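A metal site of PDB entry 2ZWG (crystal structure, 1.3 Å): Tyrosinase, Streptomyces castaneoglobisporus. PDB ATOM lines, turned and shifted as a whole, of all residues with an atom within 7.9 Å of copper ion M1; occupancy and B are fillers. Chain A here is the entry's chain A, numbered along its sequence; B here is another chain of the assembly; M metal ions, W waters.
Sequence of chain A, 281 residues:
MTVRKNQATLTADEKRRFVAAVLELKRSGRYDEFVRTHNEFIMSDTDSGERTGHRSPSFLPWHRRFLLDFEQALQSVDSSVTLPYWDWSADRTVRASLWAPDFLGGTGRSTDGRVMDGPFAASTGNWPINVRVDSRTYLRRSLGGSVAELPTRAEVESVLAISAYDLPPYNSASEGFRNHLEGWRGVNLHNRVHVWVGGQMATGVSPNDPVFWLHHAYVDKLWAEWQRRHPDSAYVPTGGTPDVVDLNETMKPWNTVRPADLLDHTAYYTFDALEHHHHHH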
ATOM      1  N   HIS A  38     -13.670  -7.114 -31.043  1.00  0.00           N
ATOM      2  CA  HIS A  38     -12.728  -7.769 -30.134  1.00  0.00           C
ATOM      3  C   HIS A  38     -12.597  -7.029 -28.816  1.00  0.00           C
ATOM      4  O   HIS A  38     -12.577  -7.641 -27.725  1.00  0.00           O
ATOM      5  CB  HIS A  38     -11.349  -7.923 -30.828  1.00  0.00           C
ATOM      6  CG  HIS A  38     -10.387  -8.684 -29.969  1.00  0.00           C
ATOM      7  ND1 HIS A  38      -9.496  -8.051 -29.156  1.00  0.00           N
ATOM      8  CD2 HIS A  38     -10.192 -10.016 -29.775  1.00  0.00           C
ATOM      9  CE1 HIS A  38      -8.761  -8.941 -28.480  1.00  0.00           C
ATOM     10  NE2 HIS A  38      -9.175 -10.149 -28.847  1.00  0.00           N
ATOM     11  N   ASN A  39     -12.472  -5.699 -28.855  1.00  0.00           N
ATOM     12  CA  ASN A  39     -12.330  -4.920 -27.633  1.00  0.00           C
ATOM     13  C   ASN A  39     -13.552  -5.054 -26.742  1.00  0.00           C
ATOM     14  O   ASN A  39     -13.445  -5.164 -25.513  1.00  0.00           O
ATOM     15  CB  ASN A  39     -12.072  -3.466 -28.025  1.00  0.00           C
ATOM     16  CG  ASN A  39     -11.579  -2.627 -26.851  1.00  0.00           C
ATOM     17  OD1 ASN A  39     -10.747  -3.087 -26.061  1.00  0.00           O
ATOM     18  ND2 ASN A  39     -12.122  -1.398 -26.766  1.00  0.00           N
ATOM     19  N   PHE A  41     -15.585  -7.576 -26.433  1.00  0.00           N
ATOM     20  CA  PHE A  41     -15.504  -8.872 -25.769  1.00  0.00           C
ATOM     21  C   PHE A  41     -14.386  -8.921 -24.753  1.00  0.00           C
ATOM     22  O   PHE A  41     -14.575  -9.407 -23.639  1.00  0.00           O
ATOM     23  CB  PHE A  41     -15.331 -10.041 -26.804  1.00  0.00           C
ATOM     24  CG  PHE A  41     -16.710 -10.404 -27.320  1.00  0.00           C
ATOM     25  CD1 PHE A  41     -17.413 -11.485 -26.794  1.00  0.00           C
ATOM     26  CD2 PHE A  41     -17.279  -9.667 -28.333  1.00  0.00           C
ATOM     27  CE1 PHE A  41     -18.689 -11.803 -27.248  1.00  0.00           C
ATOM     28  CE2 PHE A  41     -18.568  -9.946 -28.768  1.00  0.00           C
ATOM     29  CZ  PHE A  41     -19.295 -11.025 -28.239  1.00  0.00           C
ATOM     30  N   ILE A  42     -13.184  -8.412 -25.028  1.00  0.00           N
ATOM     31  CA  ILE A  42     -12.159  -8.615 -24.001  1.00  0.00           C
ATOM     32  C   ILE A  42     -12.445  -7.735 -22.813  1.00  0.00           C
ATOM     33  O   ILE A  42     -12.022  -7.992 -21.690  1.00  0.00           O
ATOM     34  CB  ILE A  42     -10.806  -8.348 -24.686  1.00  0.00           C
ATOM     35  CG1 ILE A  42      -9.658  -9.088 -23.967  1.00  0.00           C
ATOM     36  CG2 ILE A  42     -10.622  -6.850 -24.811  1.00  0.00           C
ATOM     37  CD1 ILE A  42      -8.324  -8.774 -24.603  1.00  0.00           C
ATOM     38  N   ASP A  45     -15.426 -10.166 -21.022  1.00  0.00           N
ATOM     39  CA  ASP A  45     -15.051 -11.538 -20.668  1.00  0.00           C
ATOM     40  C   ASP A  45     -14.398 -11.559 -19.292  1.00  0.00           C
ATOM     41  O   ASP A  45     -13.206 -11.220 -19.135  1.00  0.00           O
ATOM     42  CB  ASP A  45     -14.144 -12.108 -21.746  1.00  0.00           C
ATOM     43  CG  ASP A  45     -14.720 -12.457 -23.092  1.00  0.00           C
ATOM     44  OD1 ASP A  45     -13.949 -12.432 -24.104  1.00  0.00           O
ATOM     45  OD2 ASP A  45     -15.956 -12.762 -23.112  1.00  0.00           O
ATOM     46  N   GLY A  53     -15.122 -14.788 -25.340  1.00  0.00           N
ATOM     47  CA  GLY A  53     -14.041 -14.768 -26.326  1.00  0.00           C
ATOM     48  C   GLY A  53     -12.691 -15.059 -25.727  1.00  0.00           C
ATOM     49  O   GLY A  53     -11.796 -15.401 -26.492  1.00  0.00           O
ATOM     50  N   HIS A  54     -12.535 -14.887 -24.434  1.00  0.00           N
ATOM     51  CA  HIS A  54     -11.265 -15.011 -23.724  1.00  0.00           C
ATOM     52  C   HIS A  54     -11.465 -15.722 -22.407  1.00  0.00           C
ATOM     53  O   HIS A  54     -12.606 -15.819 -21.896  1.00  0.00           O
ATOM     54  CB  HIS A  54     -10.603 -13.634 -23.442  1.00  0.00           C
ATOM     55  CG  HIS A  54     -10.404 -12.901 -24.749  1.00  0.00           C
ATOM     56  ND1 HIS A  54     -11.438 -12.230 -25.378  1.00  0.00           N
ATOM     57  CD2 HIS A  54      -9.290 -12.781 -25.498  1.00  0.00           C
ATOM     58  CE1 HIS A  54     -10.925 -11.717 -26.506  1.00  0.00           C
ATOM     59  NE2 HIS A  54      -9.640 -12.018 -26.603  1.00  0.00           N
ATOM     60  N   PHE A  59     -12.569 -19.522 -25.908  1.00  0.00           N
ATOM     61  CA  PHE A  59     -11.480 -18.757 -26.480  1.00  0.00           C
ATOM     62  C   PHE A  59     -11.078 -19.257 -27.853  1.00  0.00           C
ATOM     63  O   PHE A  59     -10.939 -18.483 -28.809  1.00  0.00           O
ATOM     64  CB  PHE A  59     -10.250 -18.816 -25.551  1.00  0.00           C
ATOM     65  CG  PHE A  59      -8.963 -18.236 -26.138  1.00  0.00           C
ATOM     66  CD1 PHE A  59      -8.761 -16.899 -26.440  1.00  0.00           C
ATOM     67  CD2 PHE A  59      -7.921 -19.133 -26.351  1.00  0.00           C
ATOM     68  CE1 PHE A  59      -7.555 -16.436 -26.934  1.00  0.00           C
ATOM     69  CE2 PHE A  59      -6.689 -18.672 -26.833  1.00  0.00           C
ATOM     70  CZ  PHE A  59      -6.513 -17.331 -27.111  1.00  0.00           C
ATOM     71  N   TRP A  62     -14.183 -19.281 -30.541  1.00  0.00           N
ATOM     72  CA  TRP A  62     -14.587 -17.879 -30.775  1.00  0.00           C
ATOM     73  C   TRP A  62     -13.583 -17.187 -31.684  1.00  0.00           C
ATOM     74  O   TRP A  62     -13.938 -16.548 -32.675  1.00  0.00           O
ATOM     75  CB  TRP A  62     -14.673 -17.132 -29.446  1.00  0.00           C
ATOM     76  CG  TRP A  62     -15.337 -15.786 -29.610  1.00  0.00           C
ATOM     77  CD1 TRP A  62     -16.664 -15.529 -29.450  1.00  0.00           C
ATOM     78  CD2 TRP A  62     -14.696 -14.567 -29.987  1.00  0.00           C
ATOM     79  NE1 TRP A  62     -16.900 -14.207 -29.692  1.00  0.00           N
ATOM     80  CE2 TRP A  62     -15.713 -13.580 -30.023  1.00  0.00           C
ATOM     81  CE3 TRP A  62     -13.387 -14.154 -30.295  1.00  0.00           C
ATOM     82  CZ2 TRP A  62     -15.428 -12.262 -30.355  1.00  0.00           C
ATOM     83  CZ3 TRP A  62     -13.105 -12.831 -30.619  1.00  0.00           C
ATOM     84  CH2 TRP A  62     -14.145 -11.884 -30.651  1.00  0.00           C
ATOM     85  N   HIS A  63     -12.262 -17.320 -31.386  1.00  0.00           N
ATOM     86  CA  HIS A  63     -11.283 -16.720 -32.296  1.00  0.00           C
ATOM     87  C   HIS A  63     -11.262 -17.439 -33.631  1.00  0.00           C
ATOM     88  O   HIS A  63     -11.013 -16.805 -34.654  1.00  0.00           O
ATOM     89  CB  HIS A  63      -9.890 -16.683 -31.641  1.00  0.00           C
ATOM     90  CG  HIS A  63      -9.763 -15.578 -30.657  1.00  0.00           C
ATOM     91  ND1 HIS A  63     -10.187 -15.649 -29.327  1.00  0.00           N
ATOM     92  CD2 HIS A  63      -9.302 -14.317 -30.795  1.00  0.00           C
ATOM     93  CE1 HIS A  63      -9.968 -14.505 -28.696  1.00  0.00           C
ATOM     94  NE2 HIS A  63      -9.422 -13.665 -29.582  1.00  0.00           N
ATOM     95  N   PHE A  66     -14.189 -15.744 -35.396  1.00  0.00           N
ATOM     96  CA  PHE A  66     -13.788 -14.347 -35.670  1.00  0.00           C
ATOM     97  C   PHE A  66     -12.811 -14.256 -36.819  1.00  0.00           C
ATOM     98  O   PHE A  66     -12.912 -13.438 -37.722  1.00  0.00           O
ATOM     99  CB  PHE A  66     -13.214 -13.788 -34.385  1.00  0.00           C
ATOM    100  CG  PHE A  66     -12.870 -12.318 -34.339  1.00  0.00           C
ATOM    101  CD1 PHE A  66     -13.892 -11.382 -34.595  1.00  0.00           C
ATOM    102  CD2 PHE A  66     -11.617 -11.869 -34.003  1.00  0.00           C
ATOM    103  CE1 PHE A  66     -13.574 -10.040 -34.491  1.00  0.00           C
ATOM    104  CE2 PHE A  66     -11.314 -10.522 -33.933  1.00  0.00           C
ATOM    105  CZ  PHE A  66     -12.309  -9.590 -34.163  1.00  0.00           C
ATOM    106  N   GLU A 182      -3.730 -20.265 -24.180  1.00  0.00           N
ATOM    107  CA  GLU A 182      -4.056 -18.836 -24.024  1.00  0.00           C
ATOM    108  C   GLU A 182      -2.972 -18.095 -23.292  1.00  0.00           C
ATOM    109  O   GLU A 182      -2.521 -17.007 -23.699  1.00  0.00           O
ATOM    110  CB  GLU A 182      -5.418 -18.708 -23.321  1.00  0.00           C
ATOM    111  CG  GLU A 182      -5.894 -17.267 -23.295  1.00  0.00           C
ATOM    112  CD  GLU A 182      -7.331 -17.135 -22.799  1.00  0.00           C
ATOM    113  OE1 GLU A 182      -7.965 -18.138 -22.483  1.00  0.00           O
ATOM    114  OE2 GLU A 182      -7.788 -15.967 -22.728  1.00  0.00           O
ATOM    115  N   HIS A 190       0.025 -17.696 -26.028  1.00  0.00           N
ATOM    116  CA  HIS A 190      -0.640 -16.616 -26.773  1.00  0.00           C
ATOM    117  C   HIS A 190      -0.574 -15.245 -26.160  1.00  0.00           C
ATOM    118  O   HIS A 190      -0.360 -14.232 -26.851  1.00  0.00           O
ATOM    119  CB  HIS A 190      -2.119 -17.043 -26.975  1.00  0.00           C
ATOM    120  CG  HIS A 190      -3.086 -15.891 -27.059  1.00  0.00           C
ATOM    121  ND1 HIS A 190      -3.628 -15.300 -25.950  1.00  0.00           N
ATOM    122  CD2 HIS A 190      -3.601 -15.222 -28.120  1.00  0.00           C
ATOM    123  CE1 HIS A 190      -4.451 -14.286 -26.340  1.00  0.00           C
ATOM    124  NE2 HIS A 190      -4.451 -14.235 -27.676  1.00  0.00           N
ATOM    125  N   ASN A 191      -0.713 -15.149 -24.811  1.00  0.00           N
ATOM    126  CA  ASN A 191      -0.647 -13.835 -24.212  1.00  0.00           C
ATOM    127  C   ASN A 191       0.709 -13.157 -24.372  1.00  0.00           C
ATOM    128  O   ASN A 191       0.808 -11.957 -24.639  1.00  0.00           O
ATOM    129  CB  ASN A 191      -0.940 -13.945 -22.704  1.00  0.00           C
ATOM    130  CG  ASN A 191      -2.419 -14.087 -22.437  1.00  0.00           C
ATOM    131  OD1 ASN A 191      -3.292 -14.051 -23.309  1.00  0.00           O
ATOM    132  ND2 ASN A 191      -2.769 -14.256 -21.152  1.00  0.00           N
ATOM    133  N   HIS A 194       1.277 -11.363 -27.653  1.00  0.00           N
ATOM    134  CA  HIS A 194       0.716 -10.011 -27.667  1.00  0.00           C
ATOM    135  C   HIS A 194       1.606  -9.016 -26.962  1.00  0.00           C
ATOM    136  O   HIS A 194       1.866  -7.868 -27.383  1.00  0.00           O
ATOM    137  CB  HIS A 194      -0.644  -9.982 -26.961  1.00  0.00           C
ATOM    138  CG  HIS A 194      -1.841 -10.485 -27.729  1.00  0.00           C
ATOM    139  ND1 HIS A 194      -2.510  -9.645 -28.622  1.00  0.00           N
ATOM    140  CD2 HIS A 194      -2.511 -11.660 -27.730  1.00  0.00           C
ATOM    141  CE1 HIS A 194      -3.535 -10.328 -29.131  1.00  0.00           C
ATOM    142  NE2 HIS A 194      -3.588 -11.563 -28.622  1.00  0.00           N
ATOM    143  N   THR A 203      -3.034  -4.490 -26.288  1.00  0.00           N
ATOM    144  CA  THR A 203      -4.197  -3.851 -25.733  1.00  0.00           C
ATOM    145  C   THR A 203      -5.478  -4.521 -26.214  1.00  0.00           C
ATOM    146  O   THR A 203      -5.441  -5.397 -27.090  1.00  0.00           O
ATOM    147  CB  THR A 203      -4.325  -2.346 -26.111  1.00  0.00           C
ATOM    148  OG1 THR A 203      -4.717  -2.252 -27.505  1.00  0.00           O
ATOM    149  CG2 THR A 203      -3.002  -1.632 -25.942  1.00  0.00           C
ATOM    150  N   GLY A 204      -6.590  -4.060 -25.611  1.00  0.00           N
ATOM    151  CA  GLY A 204      -7.889  -4.568 -26.015  1.00  0.00           C
ATOM    152  C   GLY A 204      -8.188  -4.360 -27.496  1.00  0.00           C
ATOM    153  O   GLY A 204      -8.929  -5.120 -28.092  1.00  0.00           O
ATOM    154  N   SER A 206      -6.195  -4.806 -29.976  1.00  0.00           N
ATOM    155  CA  SER A 206      -5.102  -5.503 -30.647  1.00  0.00           C
ATOM    156  C   SER A 206      -5.377  -5.805 -32.104  1.00  0.00           C
ATOM    157  O   SER A 206      -4.357  -5.818 -32.818  1.00  0.00           O
ATOM    158  CB  SER A 206      -4.719  -6.793 -29.892  1.00  0.00           C
ATOM    159  OG  SER A 206      -5.870  -7.572 -29.624  1.00  0.00           O
ATOM    160  N   PRO A 207      -6.567  -6.034 -32.619  1.00  0.00           N
ATOM    161  CA  PRO A 207      -6.672  -6.195 -34.086  1.00  0.00           C
ATOM    162  C   PRO A 207      -6.316  -4.937 -34.866  1.00  0.00           C
ATOM    163  O   PRO A 207      -6.267  -5.022 -36.107  1.00  0.00           O
ATOM    164  CB  PRO A 207      -8.142  -6.560 -34.324  1.00  0.00           C
ATOM    165  CG  PRO A 207      -8.551  -7.145 -32.984  1.00  0.00           C
ATOM    166  CD  PRO A 207      -7.881  -6.251 -31.988  1.00  0.00           C
ATOM    167  N   PHE A 212      -2.230  -9.257 -35.666  1.00  0.00           N
ATOM    168  CA  PHE A 212      -3.223  -9.966 -34.867  1.00  0.00           C
ATOM    169  C   PHE A 212      -3.690 -11.241 -35.537  1.00  0.00           C
ATOM    170  O   PHE A 212      -3.834 -12.293 -34.957  1.00  0.00           O
ATOM    171  CB  PHE A 212      -4.416  -8.998 -34.635  1.00  0.00           C
ATOM    172  CG  PHE A 212      -5.573  -9.634 -33.872  1.00  0.00           C
ATOM    173  CD1 PHE A 212      -6.622 -10.318 -34.515  1.00  0.00           C
ATOM    174  CD2 PHE A 212      -5.589  -9.528 -32.480  1.00  0.00           C
ATOM    175  CE1 PHE A 212      -7.609 -10.924 -33.804  1.00  0.00           C
ATOM    176  CE2 PHE A 212      -6.603 -10.146 -31.797  1.00  0.00           C
ATOM    177  CZ  PHE A 212      -7.620 -10.824 -32.406  1.00  0.00           C
ATOM    178  N   HIS A 215      -0.994 -14.013 -35.830  1.00  0.00           N
ATOM    179  CA  HIS A 215      -0.791 -14.616 -34.509  1.00  0.00           C
ATOM    180  C   HIS A 215      -1.957 -15.560 -34.267  1.00  0.00           C
ATOM    181  O   HIS A 215      -1.757 -16.747 -33.964  1.00  0.00           O
ATOM    182  CB  HIS A 215      -0.781 -13.512 -33.460  1.00  0.00           C
ATOM    183  CG  HIS A 215      -0.749 -13.992 -32.048  1.00  0.00           C
ATOM    184  ND1 HIS A 215      -0.048 -15.169 -31.753  1.00  0.00           N
ATOM    185  CD2 HIS A 215      -1.315 -13.495 -30.926  1.00  0.00           C
ATOM    186  CE1 HIS A 215      -0.207 -15.343 -30.426  1.00  0.00           C
ATOM    187  NE2 HIS A 215      -0.941 -14.372 -29.900  1.00  0.00           N
ATOM    188  N   HIS A 216      -3.216 -15.092 -34.367  1.00  0.00           N
ATOM    189  CA  HIS A 216      -4.337 -15.996 -34.045  1.00  0.00           C
ATOM    190  C   HIS A 216      -4.446 -17.129 -35.040  1.00  0.00           C
ATOM    191  O   HIS A 216      -4.932 -18.199 -34.671  1.00  0.00           O
ATOM    192  CB  HIS A 216      -5.688 -15.209 -33.872  1.00  0.00           C
ATOM    193  CG  HIS A 216      -5.748 -14.767 -32.438  1.00  0.00           C
ATOM    194  ND1 HIS A 216      -6.225 -15.641 -31.490  1.00  0.00           N
ATOM    195  CD2 HIS A 216      -5.389 -13.639 -31.791  1.00  0.00           C
ATOM    196  CE1 HIS A 216      -6.153 -15.053 -30.284  1.00  0.00           C
ATOM    197  NE2 HIS A 216      -5.670 -13.826 -30.442  1.00  0.00           N
ATOM    198  N   DAH B  98      -3.106  -8.452 -21.805  1.00  0.00           N
ATOM    199  CA  DAH B  98      -2.620  -9.796 -21.813  1.00  0.00           C
ATOM    200  C   DAH B  98      -1.448  -9.989 -20.847  1.00  0.00           C
ATOM    201  O   DAH B  98      -0.634 -10.897 -20.993  1.00  0.00           O
ATOM    202  CB  DAH B  98      -2.141 -10.154 -23.248  1.00  0.00           C
ATOM    203  CG  DAH B  98      -3.184  -9.848 -24.311  1.00  0.00           C
ATOM    204  CD1 DAH B  98      -3.204  -8.630 -24.988  1.00  0.00           C
ATOM    205  CD2 DAH B  98      -4.132 -10.823 -24.639  1.00  0.00           C
ATOM    206  CE1 DAH B  98      -4.138  -8.347 -25.955  1.00  0.00           C
ATOM    207  CE2 DAH B  98      -5.075 -10.546 -25.606  1.00  0.00           C
ATOM    208  CZ  DAH B  98      -5.071  -9.327 -26.249  1.00  0.00           C
ATOM    209  OE2 DAH B  98      -6.050 -11.345 -26.032  1.00  0.00           O
ATOM    210  OH  DAH B  98      -6.022  -9.130 -27.218  1.00  0.00           O
HETATM  211 CU    CU M   1      -8.350 -11.863 -28.182  1.00  0.00          CU
HETATM  212 CU    CU M   2      -5.270 -12.758 -28.612  1.00  0.00          CU
HETATM  213  O   HOH W   1      -6.630 -11.356 -28.888  1.00  0.00           O
HETATM  214  O   HOH W   2      -7.171 -13.201 -27.442  1.00  0.00           O
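A ring nitrogen (ND1) of His 38 lies within hydrogen-bond range of the backbone carbonyl oxygen (O) of Gly 204 (3.2 Å).
ND1 of His 54 is in hydrogen-bond range of OD1 of Asp 45, 2.8 Å away.
The backbone carbonyl oxygen (O) of Phe 59 is in hydrogen-bond range of a ring nitrogen (ND1) of His 63 (3.0 Å).
A ring nitrogen (ND1) of His 63 sits close to the backbone carbonyl oxygen (O) of Gly 53 (3.3 Å).
OH of DAH 98 of chain B sits at hydrogen-bond distance from OG of Ser 206, 2.9 Å away.
Merely in contact with copper ion M1: DAH 98 of chain B (3.2 Å).
Four residues have an atom within 4 Å of copper ion M1: His 38, His 54, His 63 and DAH 98 of chain B.
The nearest printed residue that does not touch copper ion M1 is His 216 (4.02 Å).
Water W1 is bound to copper ion M1.
Water W2 binds copper ion M1.
NE2 of His 38 binds copper ion M1, at 2.0 Å.
A ring nitrogen (NE2) of His 54 is bound to copper ion M1 (2.0 Å).
Copper ion M1 is bound by a ring nitrogen (NE2) of His 63 (2.5 Å).
Copper ion M1 has five donor atoms within binding distance.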
